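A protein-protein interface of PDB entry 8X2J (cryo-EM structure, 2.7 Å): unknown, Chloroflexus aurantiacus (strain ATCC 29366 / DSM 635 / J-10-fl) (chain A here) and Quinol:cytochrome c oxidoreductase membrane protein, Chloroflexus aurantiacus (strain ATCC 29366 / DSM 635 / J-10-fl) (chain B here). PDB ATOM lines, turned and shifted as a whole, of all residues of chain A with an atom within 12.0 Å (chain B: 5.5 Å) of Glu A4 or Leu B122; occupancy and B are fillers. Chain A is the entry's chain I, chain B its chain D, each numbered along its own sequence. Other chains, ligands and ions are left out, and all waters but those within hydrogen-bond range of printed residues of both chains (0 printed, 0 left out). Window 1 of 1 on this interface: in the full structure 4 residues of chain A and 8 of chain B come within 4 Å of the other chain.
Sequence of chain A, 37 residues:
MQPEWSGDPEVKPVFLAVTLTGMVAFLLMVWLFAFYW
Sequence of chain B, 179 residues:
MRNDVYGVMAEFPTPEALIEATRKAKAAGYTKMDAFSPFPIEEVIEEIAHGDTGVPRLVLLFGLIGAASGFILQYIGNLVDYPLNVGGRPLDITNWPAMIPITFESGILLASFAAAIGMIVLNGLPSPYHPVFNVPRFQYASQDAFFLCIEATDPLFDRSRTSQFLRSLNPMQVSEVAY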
ATOM      1  N   MET A   1      22.797  12.910 -32.069  1.00  0.00           N
ATOM      2  CA  MET A   1      22.516  11.880 -31.079  1.00  0.00           C
ATOM      3  C   MET A   1      22.305  12.490 -29.701  1.00  0.00           C
ATOM      4  O   MET A   1      22.676  13.638 -29.454  1.00  0.00           O
ATOM      5  CB  MET A   1      23.652  10.854 -31.034  1.00  0.00           C
ATOM      6  CG  MET A   1      24.985  11.418 -30.577  1.00  0.00           C
ATOM      7  SD  MET A   1      26.323  10.213 -30.680  1.00  0.00           S
ATOM      8  CE  MET A   1      27.753  11.272 -30.491  1.00  0.00           C
ATOM      9  N   GLN A   2      21.696  11.713 -28.810  1.00  0.00           N
ATOM     10  CA  GLN A   2      21.434  12.176 -27.460  1.00  0.00           C
ATOM     11  C   GLN A   2      22.734  12.235 -26.655  1.00  0.00           C
ATOM     12  O   GLN A   2      23.689  11.516 -26.959  1.00  0.00           O
ATOM     13  CB  GLN A   2      20.430  11.251 -26.773  1.00  0.00           C
ATOM     14  CG  GLN A   2      19.029  11.319 -27.358  1.00  0.00           C
ATOM     15  CD  GLN A   2      18.250  12.525 -26.869  1.00  0.00           C
ATOM     16  OE1 GLN A   2      18.629  13.168 -25.891  1.00  0.00           O
ATOM     17  NE2 GLN A   2      17.155  12.836 -27.552  1.00  0.00           N
ATOM     18  N   PRO A   3      22.803  13.093 -25.637  1.00  0.00           N
ATOM     19  CA  PRO A   3      23.978  13.103 -24.757  1.00  0.00           C
ATOM     20  C   PRO A   3      24.032  11.869 -23.868  1.00  0.00           C
ATOM     21  O   PRO A   3      23.126  11.033 -23.837  1.00  0.00           O
ATOM     22  CB  PRO A   3      23.796  14.376 -23.928  1.00  0.00           C
ATOM     23  CG  PRO A   3      22.348  14.681 -24.007  1.00  0.00           C
ATOM     24  CD  PRO A   3      21.927  14.248 -25.374  1.00  0.00           C
ATOM     25  N   GLU A   4      25.142  11.768 -23.131  1.00  0.00           N
ATOM     26  CA  GLU A   4      25.376  10.610 -22.274  1.00  0.00           C
ATOM     27  C   GLU A   4      24.426  10.588 -21.085  1.00  0.00           C
ATOM     28  O   GLU A   4      23.898   9.531 -20.722  1.00  0.00           O
ATOM     29  CB  GLU A   4      26.827  10.605 -21.798  1.00  0.00           C
ATOM     30  CG  GLU A   4      27.198   9.441 -20.900  1.00  0.00           C
ATOM     31  CD  GLU A   4      27.587   8.207 -21.685  1.00  0.00           C
ATOM     32  OE1 GLU A   4      27.972   8.353 -22.865  1.00  0.00           O
ATOM     33  OE2 GLU A   4      27.511   7.095 -21.122  1.00  0.00           O
ATOM     34  N   TRP A   5      24.186  11.745 -20.475  1.00  0.00           N
ATOM     35  CA  TRP A   5      23.351  11.842 -19.289  1.00  0.00           C
ATOM     36  C   TRP A   5      21.893  12.150 -19.612  1.00  0.00           C
ATOM     37  O   TRP A   5      21.163  12.615 -18.731  1.00  0.00           O
ATOM     38  CB  TRP A   5      23.916  12.900 -18.338  1.00  0.00           C
ATOM     39  CG  TRP A   5      24.621  14.025 -19.030  1.00  0.00           C
ATOM     40  CD1 TRP A   5      25.967  14.196 -19.144  1.00  0.00           C
ATOM     41  CD2 TRP A   5      24.018  15.137 -19.701  1.00  0.00           C
ATOM     42  NE1 TRP A   5      26.241  15.345 -19.844  1.00  0.00           N
ATOM     43  CE2 TRP A   5      25.061  15.941 -20.198  1.00  0.00           C
ATOM     44  CE3 TRP A   5      22.695  15.529 -19.932  1.00  0.00           C
ATOM     45  CZ2 TRP A   5      24.825  17.113 -20.910  1.00  0.00           C
ATOM     46  CZ3 TRP A   5      22.463  16.692 -20.639  1.00  0.00           C
ATOM     47  CH2 TRP A   5      23.523  17.471 -21.119  1.00  0.00           C
ATOM     48  N   SER A   6      21.454  11.903 -20.844  1.00  0.00           N
ATOM     49  CA  SER A   6      20.069  12.168 -21.210  1.00  0.00           C
ATOM     50  C   SER A   6      19.141  11.171 -20.527  1.00  0.00           C
ATOM     51  O   SER A   6      19.371   9.960 -20.568  1.00  0.00           O
ATOM     52  CB  SER A   6      19.898  12.103 -22.727  1.00  0.00           C
ATOM     53  OG  SER A   6      20.299  10.842 -23.234  1.00  0.00           O
ATOM     54  N   GLY A   7      18.091  11.687 -19.894  1.00  0.00           N
ATOM     55  CA  GLY A   7      17.176  10.866 -19.132  1.00  0.00           C
ATOM     56  C   GLY A   7      17.512  10.713 -17.667  1.00  0.00           C
ATOM     57  O   GLY A   7      16.838   9.943 -16.972  1.00  0.00           O
ATOM     58  N   ASP A   8      18.531  11.421 -17.170  1.00  0.00           N
ATOM     59  CA  ASP A   8      18.936  11.360 -15.771  1.00  0.00           C
ATOM     60  C   ASP A   8      18.221  12.440 -14.977  1.00  0.00           C
ATOM     61  O   ASP A   8      18.233  13.608 -15.389  1.00  0.00           O
ATOM     62  CB  ASP A   8      20.446  11.540 -15.642  1.00  0.00           C
ATOM     63  CG  ASP A   8      21.042  10.702 -14.528  1.00  0.00           C
ATOM     64  OD1 ASP A   8      20.375   9.752 -14.071  1.00  0.00           O
ATOM     65  OD2 ASP A   8      22.181  10.994 -14.108  1.00  0.00           O
ATOM     66  N   PRO A   9      17.585  12.101 -13.849  1.00  0.00           N
ATOM     67  CA  PRO A   9      16.865  13.121 -13.068  1.00  0.00           C
ATOM     68  C   PRO A   9      17.765  14.113 -12.345  1.00  0.00           C
ATOM     69  O   PRO A   9      17.249  15.108 -11.822  1.00  0.00           O
ATOM     70  CB  PRO A   9      16.052  12.289 -12.065  1.00  0.00           C
ATOM     71  CG  PRO A   9      16.015  10.907 -12.640  1.00  0.00           C
ATOM     72  CD  PRO A   9      17.317  10.743 -13.350  1.00  0.00           C
ATOM     73  N   GLU A  10      19.075  13.880 -12.286  1.00  0.00           N
ATOM     74  CA  GLU A  10      19.999  14.796 -11.632  1.00  0.00           C
ATOM     75  C   GLU A  10      20.538  15.874 -12.566  1.00  0.00           C
ATOM     76  O   GLU A  10      21.255  16.766 -12.102  1.00  0.00           O
ATOM     77  CB  GLU A  10      21.172  14.012 -11.029  1.00  0.00           C
ATOM     78  CG  GLU A  10      21.702  14.564  -9.710  1.00  0.00           C
ATOM     79  CD  GLU A  10      20.720  14.403  -8.568  1.00  0.00           C
ATOM     80  OE1 GLU A  10      19.997  13.386  -8.539  1.00  0.00           O
ATOM     81  OE2 GLU A  10      20.673  15.296  -7.697  1.00  0.00           O
ATOM     82  N   VAL A  11      20.193  15.821 -13.856  1.00  0.00           N
ATOM     83  CA  VAL A  11      20.804  16.707 -14.846  1.00  0.00           C
ATOM     84  C   VAL A  11      20.323  18.142 -14.665  1.00  0.00           C
ATOM     85  O   VAL A  11      21.123  19.084 -14.651  1.00  0.00           O
ATOM     86  CB  VAL A  11      20.522  16.180 -16.264  1.00  0.00           C
ATOM     87  CG1 VAL A  11      20.697  17.268 -17.318  1.00  0.00           C
ATOM     88  CG2 VAL A  11      21.437  15.028 -16.552  1.00  0.00           C
ATOM     89  N   LYS A  12      19.021  18.333 -14.504  1.00  0.00           N
ATOM     90  CA  LYS A  12      18.538  19.695 -14.307  1.00  0.00           C
ATOM     91  C   LYS A  12      18.837  20.228 -12.898  1.00  0.00           C
ATOM     92  O   LYS A  12      19.126  21.426 -12.787  1.00  0.00           O
ATOM     93  CB  LYS A  12      17.045  19.797 -14.656  1.00  0.00           C
ATOM     94  CG  LYS A  12      16.762  19.747 -16.148  1.00  0.00           C
ATOM     95  CD  LYS A  12      15.377  20.276 -16.481  1.00  0.00           C
ATOM     96  CE  LYS A  12      15.127  20.244 -17.982  1.00  0.00           C
ATOM     97  NZ  LYS A  12      13.834  20.885 -18.349  1.00  0.00           N
ATOM     98  N   VAL A  14      21.690  19.555 -11.359  1.00  0.00           N
ATOM     99  CA  VAL A  14      23.099  19.940 -11.394  1.00  0.00           C
ATOM    100  C   VAL A  14      23.314  21.129 -12.336  1.00  0.00           C
ATOM    101  O   VAL A  14      24.212  21.944 -12.103  1.00  0.00           O
ATOM    102  CB  VAL A  14      24.006  18.734 -11.733  1.00  0.00           C
ATOM    103  CG1 VAL A  14      23.953  18.347 -13.199  1.00  0.00           C
ATOM    104  CG2 VAL A  14      25.441  18.996 -11.303  1.00  0.00           C
ATOM    105  N   PHE A  15      22.467  21.299 -13.361  1.00  0.00           N
ATOM    106  CA  PHE A  15      22.554  22.495 -14.195  1.00  0.00           C
ATOM    107  C   PHE A  15      22.121  23.740 -13.434  1.00  0.00           C
ATOM    108  O   PHE A  15      22.756  24.795 -13.556  1.00  0.00           O
ATOM    109  CB  PHE A  15      21.718  22.328 -15.466  1.00  0.00           C
ATOM    110  CG  PHE A  15      22.386  21.509 -16.539  1.00  0.00           C
ATOM    111  CD1 PHE A  15      23.725  21.159 -16.442  1.00  0.00           C
ATOM    112  CD2 PHE A  15      21.673  21.104 -17.658  1.00  0.00           C
ATOM    113  CE1 PHE A  15      24.337  20.413 -17.434  1.00  0.00           C
ATOM    114  CE2 PHE A  15      22.278  20.357 -18.653  1.00  0.00           C
ATOM    115  CZ  PHE A  15      23.612  20.013 -18.540  1.00  0.00           C
ATOM    116  N   ASP B  34      27.007   0.086 -26.662  1.00  0.00           N
ATOM    117  CA  ASP B  34      28.284   0.768 -26.796  1.00  0.00           C
ATOM    118  C   ASP B  34      29.377  -0.240 -27.117  1.00  0.00           C
ATOM    119  O   ASP B  34      29.316  -1.400 -26.705  1.00  0.00           O
ATOM    120  CB  ASP B  34      28.644   1.539 -25.522  1.00  0.00           C
ATOM    121  CG  ASP B  34      29.522   2.742 -25.795  1.00  0.00           C
ATOM    122  OD1 ASP B  34      30.048   2.855 -26.921  1.00  0.00           O
ATOM    123  OD2 ASP B  34      29.682   3.580 -24.884  1.00  0.00           O
ATOM    124  N   THR B  53      27.056  15.349 -32.622  1.00  0.00           N
ATOM    125  CA  THR B  53      27.782  15.172 -31.370  1.00  0.00           C
ATOM    126  C   THR B  53      27.361  16.190 -30.317  1.00  0.00           C
ATOM    127  O   THR B  53      27.415  15.896 -29.118  1.00  0.00           O
ATOM    128  CB  THR B  53      29.286  15.267 -31.622  1.00  0.00           C
ATOM    129  OG1 THR B  53      29.639  16.629 -31.887  1.00  0.00           O
ATOM    130  CG2 THR B  53      29.678  14.417 -32.813  1.00  0.00           C
ATOM    131  N   GLY B  54      26.938  17.380 -30.738  1.00  0.00           N
ATOM    132  CA  GLY B  54      26.618  18.455 -29.825  1.00  0.00           C
ATOM    133  C   GLY B  54      27.775  19.374 -29.509  1.00  0.00           C
ATOM    134  O   GLY B  54      27.560  20.423 -28.889  1.00  0.00           O
ATOM    135  N   VAL B  55      28.994  18.999 -29.896  1.00  0.00           N
ATOM    136  CA  VAL B  55      30.150  19.888 -29.728  1.00  0.00           C
ATOM    137  C   VAL B  55      30.076  21.178 -30.556  1.00  0.00           C
ATOM    138  O   VAL B  55      30.274  22.258 -29.975  1.00  0.00           O
ATOM    139  CB  VAL B  55      31.450  19.113 -29.953  1.00  0.00           C
ATOM    140  CG1 VAL B  55      32.641  19.912 -29.457  1.00  0.00           C
ATOM    141  CG2 VAL B  55      31.396  17.771 -29.247  1.00  0.00           C
ATOM    142  N   LEU B  58      27.978  24.253 -29.266  1.00  0.00           N
ATOM    143  CA  LEU B  58      28.601  24.918 -28.127  1.00  0.00           C
ATOM    144  C   LEU B  58      29.835  25.705 -28.548  1.00  0.00           C
ATOM    145  O   LEU B  58      30.095  26.789 -28.009  1.00  0.00           O
ATOM    146  CB  LEU B  58      28.966  23.891 -27.058  1.00  0.00           C
ATOM    147  CG  LEU B  58      27.796  23.165 -26.397  1.00  0.00           C
ATOM    148  CD1 LEU B  58      28.309  22.099 -25.450  1.00  0.00           C
ATOM    149  CD2 LEU B  58      26.904  24.151 -25.667  1.00  0.00           C
ATOM    150  N   ILE B 117      35.485  21.390 -22.822  1.00  0.00           N
ATOM    151  CA  ILE B 117      34.568  21.137 -21.714  1.00  0.00           C
ATOM    152  C   ILE B 117      33.252  20.555 -22.219  1.00  0.00           C
ATOM    153  O   ILE B 117      32.665  19.678 -21.574  1.00  0.00           O
ATOM    154  CB  ILE B 117      34.359  22.427 -20.896  1.00  0.00           C
ATOM    155  CG1 ILE B 117      35.705  22.996 -20.442  1.00  0.00           C
ATOM    156  CG2 ILE B 117      33.489  22.180 -19.674  1.00  0.00           C
ATOM    157  CD1 ILE B 117      36.512  22.053 -19.584  1.00  0.00           C
ATOM    158  N   GLY B 118      32.791  20.991 -23.396  1.00  0.00           N
ATOM    159  CA  GLY B 118      31.586  20.431 -23.970  1.00  0.00           C
ATOM    160  C   GLY B 118      31.741  18.983 -24.378  1.00  0.00           C
ATOM    161  O   GLY B 118      30.830  18.188 -24.161  1.00  0.00           O
ATOM    162  N   MET B 119      32.901  18.609 -24.939  1.00  0.00           N
ATOM    163  CA  MET B 119      33.136  17.200 -25.246  1.00  0.00           C
ATOM    164  C   MET B 119      33.187  16.358 -23.979  1.00  0.00           C
ATOM    165  O   MET B 119      32.523  15.316 -23.899  1.00  0.00           O
ATOM    166  CB  MET B 119      34.429  17.035 -26.033  1.00  0.00           C
ATOM    167  CG  MET B 119      34.684  15.607 -26.485  1.00  0.00           C
ATOM    168  SD  MET B 119      35.976  14.767 -25.551  1.00  0.00           S
ATOM    169  CE  MET B 119      37.423  15.667 -26.096  1.00  0.00           C
ATOM    170  N   ILE B 120      33.930  16.831 -22.967  1.00  0.00           N
ATOM    171  CA  ILE B 120      34.122  16.083 -21.722  1.00  0.00           C
ATOM    172  C   ILE B 120      32.794  15.892 -20.992  1.00  0.00           C
ATOM    173  O   ILE B 120      32.489  14.795 -20.510  1.00  0.00           O
ATOM    174  CB  ILE B 120      35.166  16.792 -20.831  1.00  0.00           C
ATOM    175  CG1 ILE B 120      36.554  16.811 -21.481  1.00  0.00           C
ATOM    176  CG2 ILE B 120      35.284  16.133 -19.476  1.00  0.00           C
ATOM    177  CD1 ILE B 120      37.004  15.514 -22.066  1.00  0.00           C
ATOM    178  N   VAL B 121      31.972  16.943 -20.928  1.00  0.00           N
ATOM    179  CA  VAL B 121      30.670  16.840 -20.277  1.00  0.00           C
ATOM    180  C   VAL B 121      29.700  16.016 -21.122  1.00  0.00           C
ATOM    181  O   VAL B 121      28.980  15.156 -20.597  1.00  0.00           O
ATOM    182  CB  VAL B 121      30.129  18.253 -19.977  1.00  0.00           C
ATOM    183  CG1 VAL B 121      28.657  18.220 -19.597  1.00  0.00           C
ATOM    184  CG2 VAL B 121      30.939  18.894 -18.866  1.00  0.00           C
ATOM    185  N   LEU B 122      29.693  16.229 -22.443  1.00  0.00           N
ATOM    186  CA  LEU B 122      28.662  15.659 -23.302  1.00  0.00           C
ATOM    187  C   LEU B 122      28.832  14.161 -23.499  1.00  0.00           C
ATOM    188  O   LEU B 122      27.832  13.454 -23.663  1.00  0.00           O
ATOM    189  CB  LEU B 122      28.660  16.375 -24.651  1.00  0.00           C
ATOM    190  CG  LEU B 122      27.674  17.532 -24.804  1.00  0.00           C
ATOM    191  CD1 LEU B 122      27.952  18.274 -26.091  1.00  0.00           C
ATOM    192  CD2 LEU B 122      26.248  17.034 -24.770  1.00  0.00           C
ATOM    193  N   ASN B 123      30.078  13.683 -23.511  1.00  0.00           N
ATOM    194  CA  ASN B 123      30.310  12.218 -23.617  1.00  0.00           C
ATOM    195  C   ASN B 123      30.170  11.606 -22.221  1.00  0.00           C
ATOM    196  O   ASN B 123      30.188  10.368 -22.119  1.00  0.00           O
ATOM    197  CB  ASN B 123      31.659  11.889 -24.263  1.00  0.00           C
ATOM    198  CG  ASN B 123      32.845  12.310 -23.421  1.00  0.00           C
ATOM    199  OD1 ASN B 123      32.684  12.987 -22.409  1.00  0.00           O
ATOM    200  ND2 ASN B 123      34.039  11.916 -23.831  1.00  0.00           N
ATOM    201  N   GLY B 124      30.015  12.445 -21.193  1.00  0.00           N
ATOM    202  CA  GLY B 124      29.936  11.941 -19.809  1.00  0.00           C
ATOM    203  C   GLY B 124      31.263  11.345 -19.372  1.00  0.00           C
ATOM    204  O   GLY B 124      31.247  10.389 -18.572  1.00  0.00           O
ATOM    205  N   HIS B 130      33.423   3.378 -13.741  1.00  0.00           N
ATOM    206  CA  HIS B 130      32.348   2.970 -14.624  1.00  0.00           C
ATOM    207  C   HIS B 130      32.076   1.502 -14.349  1.00  0.00           C
ATOM    208  O   HIS B 130      32.976   0.783 -13.898  1.00  0.00           O
ATOM    209  CB  HIS B 130      32.698   3.180 -16.105  1.00  0.00           C
ATOM    210  CG  HIS B 130      31.500   3.320 -16.991  1.00  0.00           C
ATOM    211  ND1 HIS B 130      30.940   2.252 -17.657  1.00  0.00           N
ATOM    212  CD2 HIS B 130      30.741   4.396 -17.302  1.00  0.00           C
ATOM    213  CE1 HIS B 130      29.897   2.666 -18.352  1.00  0.00           C
ATOM    214  NE2 HIS B 130      29.754   3.963 -18.154  1.00  0.00           N
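Among the printed residues, pairs that only touch across the chains: Pro A3 with Leu B122 (3.7 Å), Glu A4 with Gly B124 (3.7 Å) and Met A1 with Thr B53 (3.998 Å).
Hydrophobic or aromatic side chains of chain A within 4 Å of the printed part of chain B: Met A1, Pro A3 and Trp A5.
Of the 14 printed residues of chain B, 5 touch a printed residue of chain A.
Hydrophobic or aromatic side chains of chain B that line the printed part of chain A: Val B121 and Leu B122.
Of the printed residues of chain B, Met A1 touches Thr B53 (3.998 Å).
Of the printed residues of chain B, Pro A3 touches Leu B122.
Glu A4 touches just these residues of chain B: Leu B122, Asn B123 and Gly B124.
Of the printed residues of chain B, Trp A5 touches Val B121.
Of the printed residues of chain A, Thr B53 touches Met A1 (3.998 Å).
Gly B54 touches none of the printed residues of chain A.
No residue of chain A comes within 4 Å of Val B55.
Leu B58 touches none of the printed residues of chain A.
Ile B117 touches none of the printed residues of chain A.
No residue of chain A comes within 4 Å of Ile B120.
Of chain A, only Trp A5 comes within 4 Å of Val B121.
Leu B122 touches two residues of chain A.
Asn B123 touches just one residue of chain A: Glu A4 (3.1 Å).
Of the printed residues of chain A, Gly B124 touches Glu A4.
The nearest residue of chain B that does not touch Glu A4 is His B130 (4.9 Å).
OG1 of Thr B53 lies within hydrogen-bond range of N of Val B55, at 3.2 Å.
OD1 of Asn B123 sits close to O of Met B119 (2.8 Å).
The backbone carbonyl oxygen of Ile B120 sits close to the side-chain amide oxygen of Asn B123 (2.6 Å).
The backbone carbonyl oxygen (O) of Pro A3 sits at hydrogen-bond distance from the side-chain hydroxyl (OG) of Ser A6, 2.9 Å away.
O of Val B121 is in hydrogen-bond range of NE1 of Trp A5, 2.8 Å away.
O of Leu B122 sits at hydrogen-bond distance from N of Glu A4.
The side-chain carboxylate (OE1) of Glu A4 lies close to the backbone carbonyl oxygen (O) of Asn B123 (3.1 Å).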
